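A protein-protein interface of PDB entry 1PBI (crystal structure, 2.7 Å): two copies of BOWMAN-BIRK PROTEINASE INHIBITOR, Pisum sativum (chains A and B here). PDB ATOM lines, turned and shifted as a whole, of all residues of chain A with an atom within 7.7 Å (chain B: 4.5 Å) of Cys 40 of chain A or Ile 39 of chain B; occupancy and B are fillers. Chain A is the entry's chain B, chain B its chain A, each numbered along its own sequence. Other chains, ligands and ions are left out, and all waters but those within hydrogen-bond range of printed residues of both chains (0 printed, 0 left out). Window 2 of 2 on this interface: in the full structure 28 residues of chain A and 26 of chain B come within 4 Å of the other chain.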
ATOM      1  N   GLY A  28       5.541  21.916   2.605  1.00  0.00           N
ATOM      2  CA  GLY A  28       5.327  21.411   1.260  1.00  0.00           C
ATOM      3  C   GLY A  28       6.489  21.671   0.329  1.00  0.00           C
ATOM      4  O   GLY A  28       7.526  22.172   0.753  1.00  0.00           O
ATOM      5  N   GLU A  29       6.325  21.330  -0.946  1.00  0.00           N
ATOM      6  CA  GLU A  29       7.378  21.546  -1.933  1.00  0.00           C
ATOM      7  C   GLU A  29       7.578  23.033  -2.205  1.00  0.00           C
ATOM      8  O   GLU A  29       8.514  23.437  -2.894  1.00  0.00           O
ATOM      9  CB  GLU A  29       7.028  20.840  -3.235  1.00  0.00           C
ATOM     10  CG  GLU A  29       6.674  19.376  -3.050  1.00  0.00           C
ATOM     11  CD  GLU A  29       6.776  18.580  -4.337  1.00  0.00           C
ATOM     12  OE1 GLU A  29       7.458  19.047  -5.279  1.00  0.00           O
ATOM     13  OE2 GLU A  29       6.178  17.483  -4.399  1.00  0.00           O
ATOM     14  N   THR A  30       6.688  23.842  -1.655  1.00  0.00           N
ATOM     15  CA  THR A  30       6.765  25.277  -1.822  1.00  0.00           C
ATOM     16  C   THR A  30       5.909  25.976  -0.750  1.00  0.00           C
ATOM     17  O   THR A  30       5.211  25.321   0.029  1.00  0.00           O
ATOM     18  CB  THR A  30       6.316  25.673  -3.262  1.00  0.00           C
ATOM     19  OG1 THR A  30       6.776  26.996  -3.561  1.00  0.00           O
ATOM     20  CG2 THR A  30       4.800  25.599  -3.404  1.00  0.00           C
ATOM     21  N   CYS A  31       6.000  27.300  -0.683  1.00  0.00           N
ATOM     22  CA  CYS A  31       5.238  28.080   0.292  1.00  0.00           C
ATOM     23  C   CYS A  31       4.083  28.797  -0.405  1.00  0.00           C
ATOM     24  O   CYS A  31       4.026  28.835  -1.634  1.00  0.00           O
ATOM     25  CB  CYS A  31       6.159  29.104   0.959  1.00  0.00           C
ATOM     26  SG  CYS A  31       7.545  28.340   1.844  1.00  0.00           S
ATOM     27  N   SER A  37       9.632  34.968   3.394  1.00  0.00           N
ATOM     28  CA  SER A  37      10.735  34.091   3.767  1.00  0.00           C
ATOM     29  C   SER A  37      10.338  32.619   3.795  1.00  0.00           C
ATOM     30  O   SER A  37       9.845  32.111   4.799  1.00  0.00           O
ATOM     31  CB  SER A  37      11.275  34.515   5.130  1.00  0.00           C
ATOM     32  OG  SER A  37      11.952  33.445   5.753  1.00  0.00           O
ATOM     33  N   CYS A  38      10.586  31.940   2.682  1.00  0.00           N
ATOM     34  CA  CYS A  38      10.261  30.520   2.506  1.00  0.00           C
ATOM     35  C   CYS A  38      11.505  29.653   2.716  1.00  0.00           C
ATOM     36  O   CYS A  38      12.404  29.634   1.877  1.00  0.00           O
ATOM     37  CB  CYS A  38       9.699  30.321   1.095  1.00  0.00           C
ATOM     38  SG  CYS A  38       9.141  28.652   0.661  1.00  0.00           S
ATOM     39  N   ILE A  39      11.551  28.931   3.833  1.00  0.00           N
ATOM     40  CA  ILE A  39      12.697  28.089   4.144  1.00  0.00           C
ATOM     41  C   ILE A  39      12.470  26.598   3.901  1.00  0.00           C
ATOM     42  O   ILE A  39      11.505  26.011   4.401  1.00  0.00           O
ATOM     43  CB  ILE A  39      13.104  28.275   5.595  1.00  0.00           C
ATOM     44  CG1 ILE A  39      13.049  29.754   5.961  1.00  0.00           C
ATOM     45  CG2 ILE A  39      14.490  27.726   5.808  1.00  0.00           C
ATOM     46  CD1 ILE A  39      14.204  30.555   5.380  1.00  0.00           C
ATOM     47  N   CYS A  40      13.383  25.989   3.149  1.00  0.00           N
ATOM     48  CA  CYS A  40      13.292  24.571   2.825  1.00  0.00           C
ATOM     49  C   CYS A  40      14.468  23.739   3.336  1.00  0.00           C
ATOM     50  O   CYS A  40      15.564  24.245   3.562  1.00  0.00           O
ATOM     51  CB  CYS A  40      13.233  24.370   1.307  1.00  0.00           C
ATOM     52  SG  CYS A  40      12.070  25.422   0.389  1.00  0.00           S
ATOM     53  N   ALA A  41      14.221  22.446   3.499  1.00  0.00           N
ATOM     54  CA  ALA A  41      15.242  21.506   3.915  1.00  0.00           C
ATOM     55  C   ALA A  41      15.759  20.975   2.570  1.00  0.00           C
ATOM     56  O   ALA A  41      15.033  21.013   1.569  1.00  0.00           O
ATOM     57  CB  ALA A  41      14.613  20.385   4.741  1.00  0.00           C
ATOM     58  N   TYR A  42      16.990  20.481   2.531  1.00  0.00           N
ATOM     59  CA  TYR A  42      17.551  19.980   1.277  1.00  0.00           C
ATOM     60  C   TYR A  42      17.368  18.477   1.037  1.00  0.00           C
ATOM     61  O   TYR A  42      18.343  17.738   0.914  1.00  0.00           O
ATOM     62  CB  TYR A  42      19.035  20.349   1.186  1.00  0.00           C
ATOM     63  N   SER A  43      16.120  18.034   0.959  1.00  0.00           N
ATOM     64  CA  SER A  43      15.817  16.627   0.707  1.00  0.00           C
ATOM     65  C   SER A  43      14.901  16.521  -0.512  1.00  0.00           C
ATOM     66  O   SER A  43      14.339  17.522  -0.959  1.00  0.00           O
ATOM     67  CB  SER A  43      15.137  15.997   1.928  1.00  0.00           C
ATOM     68  OG  SER A  43      14.341  16.935   2.629  1.00  0.00           O
ATOM     69  N   PRO A  46      11.478  18.330  -1.776  1.00  0.00           N
ATOM     70  CA  PRO A  46      11.727  19.383  -0.781  1.00  0.00           C
ATOM     71  C   PRO A  46      10.656  19.546   0.272  1.00  0.00           C
ATOM     72  O   PRO A  46       9.507  19.147   0.083  1.00  0.00           O
ATOM     73  CB  PRO A  46      11.873  20.650  -1.613  1.00  0.00           C
ATOM     74  CG  PRO A  46      12.013  20.194  -3.013  1.00  0.00           C
ATOM     75  CD  PRO A  46      11.306  18.884  -3.119  1.00  0.00           C
ATOM     76  N   LYS A  47      11.054  20.135   1.394  1.00  0.00           N
ATOM     77  CA  LYS A  47      10.162  20.395   2.514  1.00  0.00           C
ATOM     78  C   LYS A  47      10.355  21.868   2.815  1.00  0.00           C
ATOM     79  O   LYS A  47      11.439  22.270   3.230  1.00  0.00           O
ATOM     80  CB  LYS A  47      10.577  19.574   3.735  1.00  0.00           C
ATOM     81  CG  LYS A  47       9.921  18.227   3.846  1.00  0.00           C
ATOM     82  CD  LYS A  47       9.456  17.975   5.259  1.00  0.00           C
ATOM     83  CE  LYS A  47      10.032  16.682   5.823  1.00  0.00           C
ATOM     84  NZ  LYS A  47       9.484  16.402   7.191  1.00  0.00           N
ATOM     85  N   CYS A  48       9.318  22.676   2.596  1.00  0.00           N
ATOM     86  CA  CYS A  48       9.415  24.110   2.852  1.00  0.00           C
ATOM     87  C   CYS A  48       8.346  24.633   3.777  1.00  0.00           C
ATOM     88  O   CYS A  48       7.222  24.140   3.813  1.00  0.00           O
ATOM     89  CB  CYS A  48       9.344  24.898   1.554  1.00  0.00           C
ATOM     90  SG  CYS A  48      10.415  24.275   0.235  1.00  0.00           S
ATOM     91  N   GLN A  49       8.714  25.648   4.537  1.00  0.00           N
ATOM     92  CA  GLN A  49       7.782  26.266   5.451  1.00  0.00           C
ATOM     93  C   GLN A  49       8.038  27.757   5.417  1.00  0.00           C
ATOM     94  O   GLN A  49       9.172  28.200   5.242  1.00  0.00           O
ATOM     95  CB  GLN A  49       7.970  25.740   6.869  1.00  0.00           C
ATOM     96  CG  GLN A  49       6.804  26.078   7.737  1.00  0.00           C
ATOM     97  CD  GLN A  49       7.029  25.741   9.176  1.00  0.00           C
ATOM     98  OE1 GLN A  49       6.974  24.579   9.552  1.00  0.00           O
ATOM     99  NE2 GLN A  49       7.283  26.754   9.999  1.00  0.00           N
ATOM    100  N   CYS A  50       6.970  28.526   5.568  1.00  0.00           N
ATOM    101  CA  CYS A  50       7.056  29.974   5.542  1.00  0.00           C
ATOM    102  C   CYS A  50       7.355  30.487   6.935  1.00  0.00           C
ATOM    103  O   CYS A  50       6.556  30.309   7.853  1.00  0.00           O
ATOM    104  CB  CYS A  50       5.740  30.565   5.048  1.00  0.00           C
ATOM    105  SG  CYS A  50       5.857  32.351   4.760  1.00  0.00           S
ATOM    106  N   PHE A  51       8.499  31.141   7.085  1.00  0.00           N
ATOM    107  CA  PHE A  51       8.917  31.665   8.377  1.00  0.00           C
ATOM    108  C   PHE A  51       8.344  33.037   8.726  1.00  0.00           C
ATOM    109  O   PHE A  51       8.593  33.556   9.813  1.00  0.00           O
ATOM    110  CB  PHE A  51      10.447  31.695   8.438  1.00  0.00           C
ATOM    111  CG  PHE A  51      11.057  30.386   8.855  1.00  0.00           C
ATOM    112  CD1 PHE A  51      10.600  29.187   8.325  1.00  0.00           C
ATOM    113  CD2 PHE A  51      12.060  30.346   9.811  1.00  0.00           C
ATOM    114  CE1 PHE A  51      11.126  27.967   8.748  1.00  0.00           C
ATOM    115  CE2 PHE A  51      12.587  29.130  10.235  1.00  0.00           C
ATOM    116  CZ  PHE A  51      12.117  27.942   9.703  1.00  0.00           C
ATOM    117  N   SER B  37      17.465  17.227  12.105  1.00  0.00           N
ATOM    118  CA  SER B  37      17.435  18.213  11.029  1.00  0.00           C
ATOM    119  C   SER B  37      16.951  19.584  11.492  1.00  0.00           C
ATOM    120  O   SER B  37      15.756  19.837  11.533  1.00  0.00           O
ATOM    121  CB  SER B  37      16.530  17.709   9.919  1.00  0.00           C
ATOM    122  OG  SER B  37      16.900  18.296   8.691  1.00  0.00           O
ATOM    123  N   CYS B  38      17.876  20.472  11.824  1.00  0.00           N
ATOM    124  CA  CYS B  38      17.531  21.812  12.301  1.00  0.00           C
ATOM    125  C   CYS B  38      17.725  22.851  11.197  1.00  0.00           C
ATOM    126  O   CYS B  38      18.847  23.127  10.788  1.00  0.00           O
ATOM    127  CB  CYS B  38      18.396  22.165  13.515  1.00  0.00           C
ATOM    128  SG  CYS B  38      18.041  23.774  14.298  1.00  0.00           S
ATOM    129  N   ILE B  39      16.625  23.430  10.729  1.00  0.00           N
ATOM    130  CA  ILE B  39      16.659  24.415   9.653  1.00  0.00           C
ATOM    131  C   ILE B  39      16.472  25.832  10.162  1.00  0.00           C
ATOM    132  O   ILE B  39      15.524  26.107  10.898  1.00  0.00           O
ATOM    133  CB  ILE B  39      15.549  24.137   8.617  1.00  0.00           C
ATOM    134  CG1 ILE B  39      15.526  22.648   8.247  1.00  0.00           C
ATOM    135  CG2 ILE B  39      15.757  25.009   7.406  1.00  0.00           C
ATOM    136  CD1 ILE B  39      16.785  22.145   7.553  1.00  0.00           C
ATOM    137  N   CYS B  40      17.374  26.725   9.755  1.00  0.00           N
ATOM    138  CA  CYS B  40      17.330  28.131  10.169  1.00  0.00           C
ATOM    139  C   CYS B  40      17.252  29.066   8.983  1.00  0.00           C
ATOM    140  O   CYS B  40      17.641  28.703   7.875  1.00  0.00           O
ATOM    141  CB  CYS B  40      18.581  28.528  10.966  1.00  0.00           C
ATOM    142  SG  CYS B  40      19.062  27.426  12.330  1.00  0.00           S
ATOM    143  N   LYS B  47      16.620  32.244  13.163  1.00  0.00           N
ATOM    144  CA  LYS B  47      15.310  31.670  13.421  1.00  0.00           C
ATOM    145  C   LYS B  47      15.426  30.232  12.968  1.00  0.00           C
ATOM    146  O   LYS B  47      15.617  29.976  11.781  1.00  0.00           O
ATOM    147  CB  LYS B  47      14.260  32.384  12.575  1.00  0.00           C
ATOM    148  CG  LYS B  47      13.324  33.287  13.357  1.00  0.00           C
ATOM    149  CD  LYS B  47      11.876  32.982  13.019  1.00  0.00           C
ATOM    150  CE  LYS B  47      11.082  34.253  12.833  1.00  0.00           C
ATOM    151  NZ  LYS B  47      11.984  35.428  12.884  1.00  0.00           N
ATOM    152  N   CYS B  48      15.319  29.292  13.902  1.00  0.00           N
ATOM    153  CA  CYS B  48      15.452  27.890  13.548  1.00  0.00           C
ATOM    154  C   CYS B  48      14.275  27.054  13.947  1.00  0.00           C
ATOM    155  O   CYS B  48      13.599  27.345  14.923  1.00  0.00           O
ATOM    156  CB  CYS B  48      16.695  27.298  14.196  1.00  0.00           C
ATOM    157  SG  CYS B  48      18.215  28.264  13.969  1.00  0.00           S
ATOM    158  N   GLN B  49      14.028  26.007  13.181  1.00  0.00           N
ATOM    159  CA  GLN B  49      12.946  25.109  13.503  1.00  0.00           C
ATOM    160  C   GLN B  49      13.420  23.698  13.233  1.00  0.00           C
ATOM    161  O   GLN B  49      14.254  23.475  12.356  1.00  0.00           O
ATOM    162  CB  GLN B  49      11.714  25.418  12.666  1.00  0.00           C
ATOM    163  CG  GLN B  49      10.445  25.248  13.450  1.00  0.00           C
ATOM    164  CD  GLN B  49       9.227  25.208  12.582  1.00  0.00           C
ATOM    165  OE1 GLN B  49       8.619  26.237  12.317  1.00  0.00           O
ATOM    166  NE2 GLN B  49       8.854  24.012  12.132  1.00  0.00           N
ATOM    167  N   PHE B  51      12.919  20.235  11.687  1.00  0.00           N
ATOM    168  CA  PHE B  51      12.101  19.610  10.656  1.00  0.00           C
ATOM    169  C   PHE B  51      11.888  18.107  10.791  1.00  0.00           C
ATOM    170  O   PHE B  51      11.340  17.480   9.889  1.00  0.00           O
ATOM    171  CB  PHE B  51      12.699  19.902   9.287  1.00  0.00           C
ATOM    172  CG  PHE B  51      12.210  21.179   8.678  1.00  0.00           C
ATOM    173  CD1 PHE B  51      12.359  22.380   9.352  1.00  0.00           C
ATOM    174  CD2 PHE B  51      11.613  21.185   7.420  1.00  0.00           C
ATOM    175  CE1 PHE B  51      11.922  23.574   8.784  1.00  0.00           C
ATOM    176  CE2 PHE B  51      11.172  22.376   6.847  1.00  0.00           C
ATOM    177  CZ  PHE B  51      11.328  23.570   7.531  1.00  0.00           C
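The side-chain amide oxygen (OE1) of Gln 49 of chain B is in hydrogen-bond range of the side-chain amide nitrogen (NE2) of Gln 49 of chain A, at 2.7 Å. The backbone carbonyl oxygen (O) of Phe 51 of chain B lies within hydrogen-bond range of the side-chain amino group (NZ) of Lys 47 of chain A (3.4 Å).
The backbone carbonyl oxygen (O) of Ser 37 of chain A lies within hydrogen-bond range of the backbone NH (N) of Phe 51 of chain A. The backbone carbonyl oxygen (O) of Lys 47 of chain A sits at hydrogen-bond distance from the backbone NH (N) of Ala 41 of chain A, at 2.8 Å. The side-chain sulfur (SG) of Cys 48 of chain A is disulfide-bonded to the side-chain sulfur (SG) of Cys 40 of chain A, at 2.0 Å. SG of Cys 40 of chain B forms a disulfide with SG of Cys 48 of chain B. O of Ile 39 of chain B lies within hydrogen-bond range of N of Gln 49 of chain B (2.7 Å). The side-chain sulfur of Cys 31 of chain A is disulfide-bonded to the side-chain sulfur of Cys 38 of chain A (2.0 Å).
CG2 of Ile 39 of chain B touches CG2 of Ile 39 of chain A (3.4 Å). CG2 of Ile 39 of chain A touches O of Cys 40 of chain B, at 3.9 Å. Ile 39 of chain A touches Phe 51 of chain B (O to CZ, 3.97 Å). Cys 40 of chain A touches Ile 39 of chain B. Ile 39 of chain B touches Ala 41 of chain A. CE2 of Phe 51 of chain A touches O of Lys 47 of chain B (3.5 Å). Phe 51 of chain A touches Gln 49 of chain B (CZ to CB, 3.9 Å).
Cys 40 of chain A touches just one residue of chain B: Ile 39. Of chain A, only Ile 39 (3.4 Å), Cys 40 (3.9 Å) and Ala 41 (3.97 Å) come within 4 Å of Ile 39 of chain B. Of the printed residues of chain B, Phe 51 of chain A touches Lys 47 (3.5 Å) and Gln 49 (3.9 Å). Printed residues of chain B within 4 Å of Gln 49 of chain A: Gln 49. Printed residues of chain A within 4 Å of Cys 40 of chain B: Ile 39. The nearest printed residue of chain B that does not touch Cys 40 of chain A is Phe 51 of chain B (5.0 Å).
Hydrophobic or aromatic side chains of chain A that line the printed part of chain B: Ile 39, Ala 41 and Phe 51. Of the 8 printed residues of chain B, 5 touch a printed residue of chain A. Among the printed residues, 9 pairs touch across the chains. Among the printed residues, no Asp or Glu carboxylate lies within 4 Å of a Lys or Arg side-chain nitrogen of the other chain.
Ile 39 of chain A touches Cys 40 of chain B, and with the chains exchanged Cys 40 of chain A touches Ile 39 of chain B. Lys 47 of chain A touches Phe 51 of chain B, and with the chains exchanged Phe 51 of chain A touches Lys 47 of chain B. Gln 49 of chain A touches its own counterpart, Gln 49 of chain B. Phe 51 of chain A touches Gln 49 of chain B, but with the chains exchanged Gln 49 of chain A does not touch Phe 51 of chain B (4.1 Å). Of the 9 pairs that touch across the chains among the printed residues, 6 have their exchanged pair printed and touching as well.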
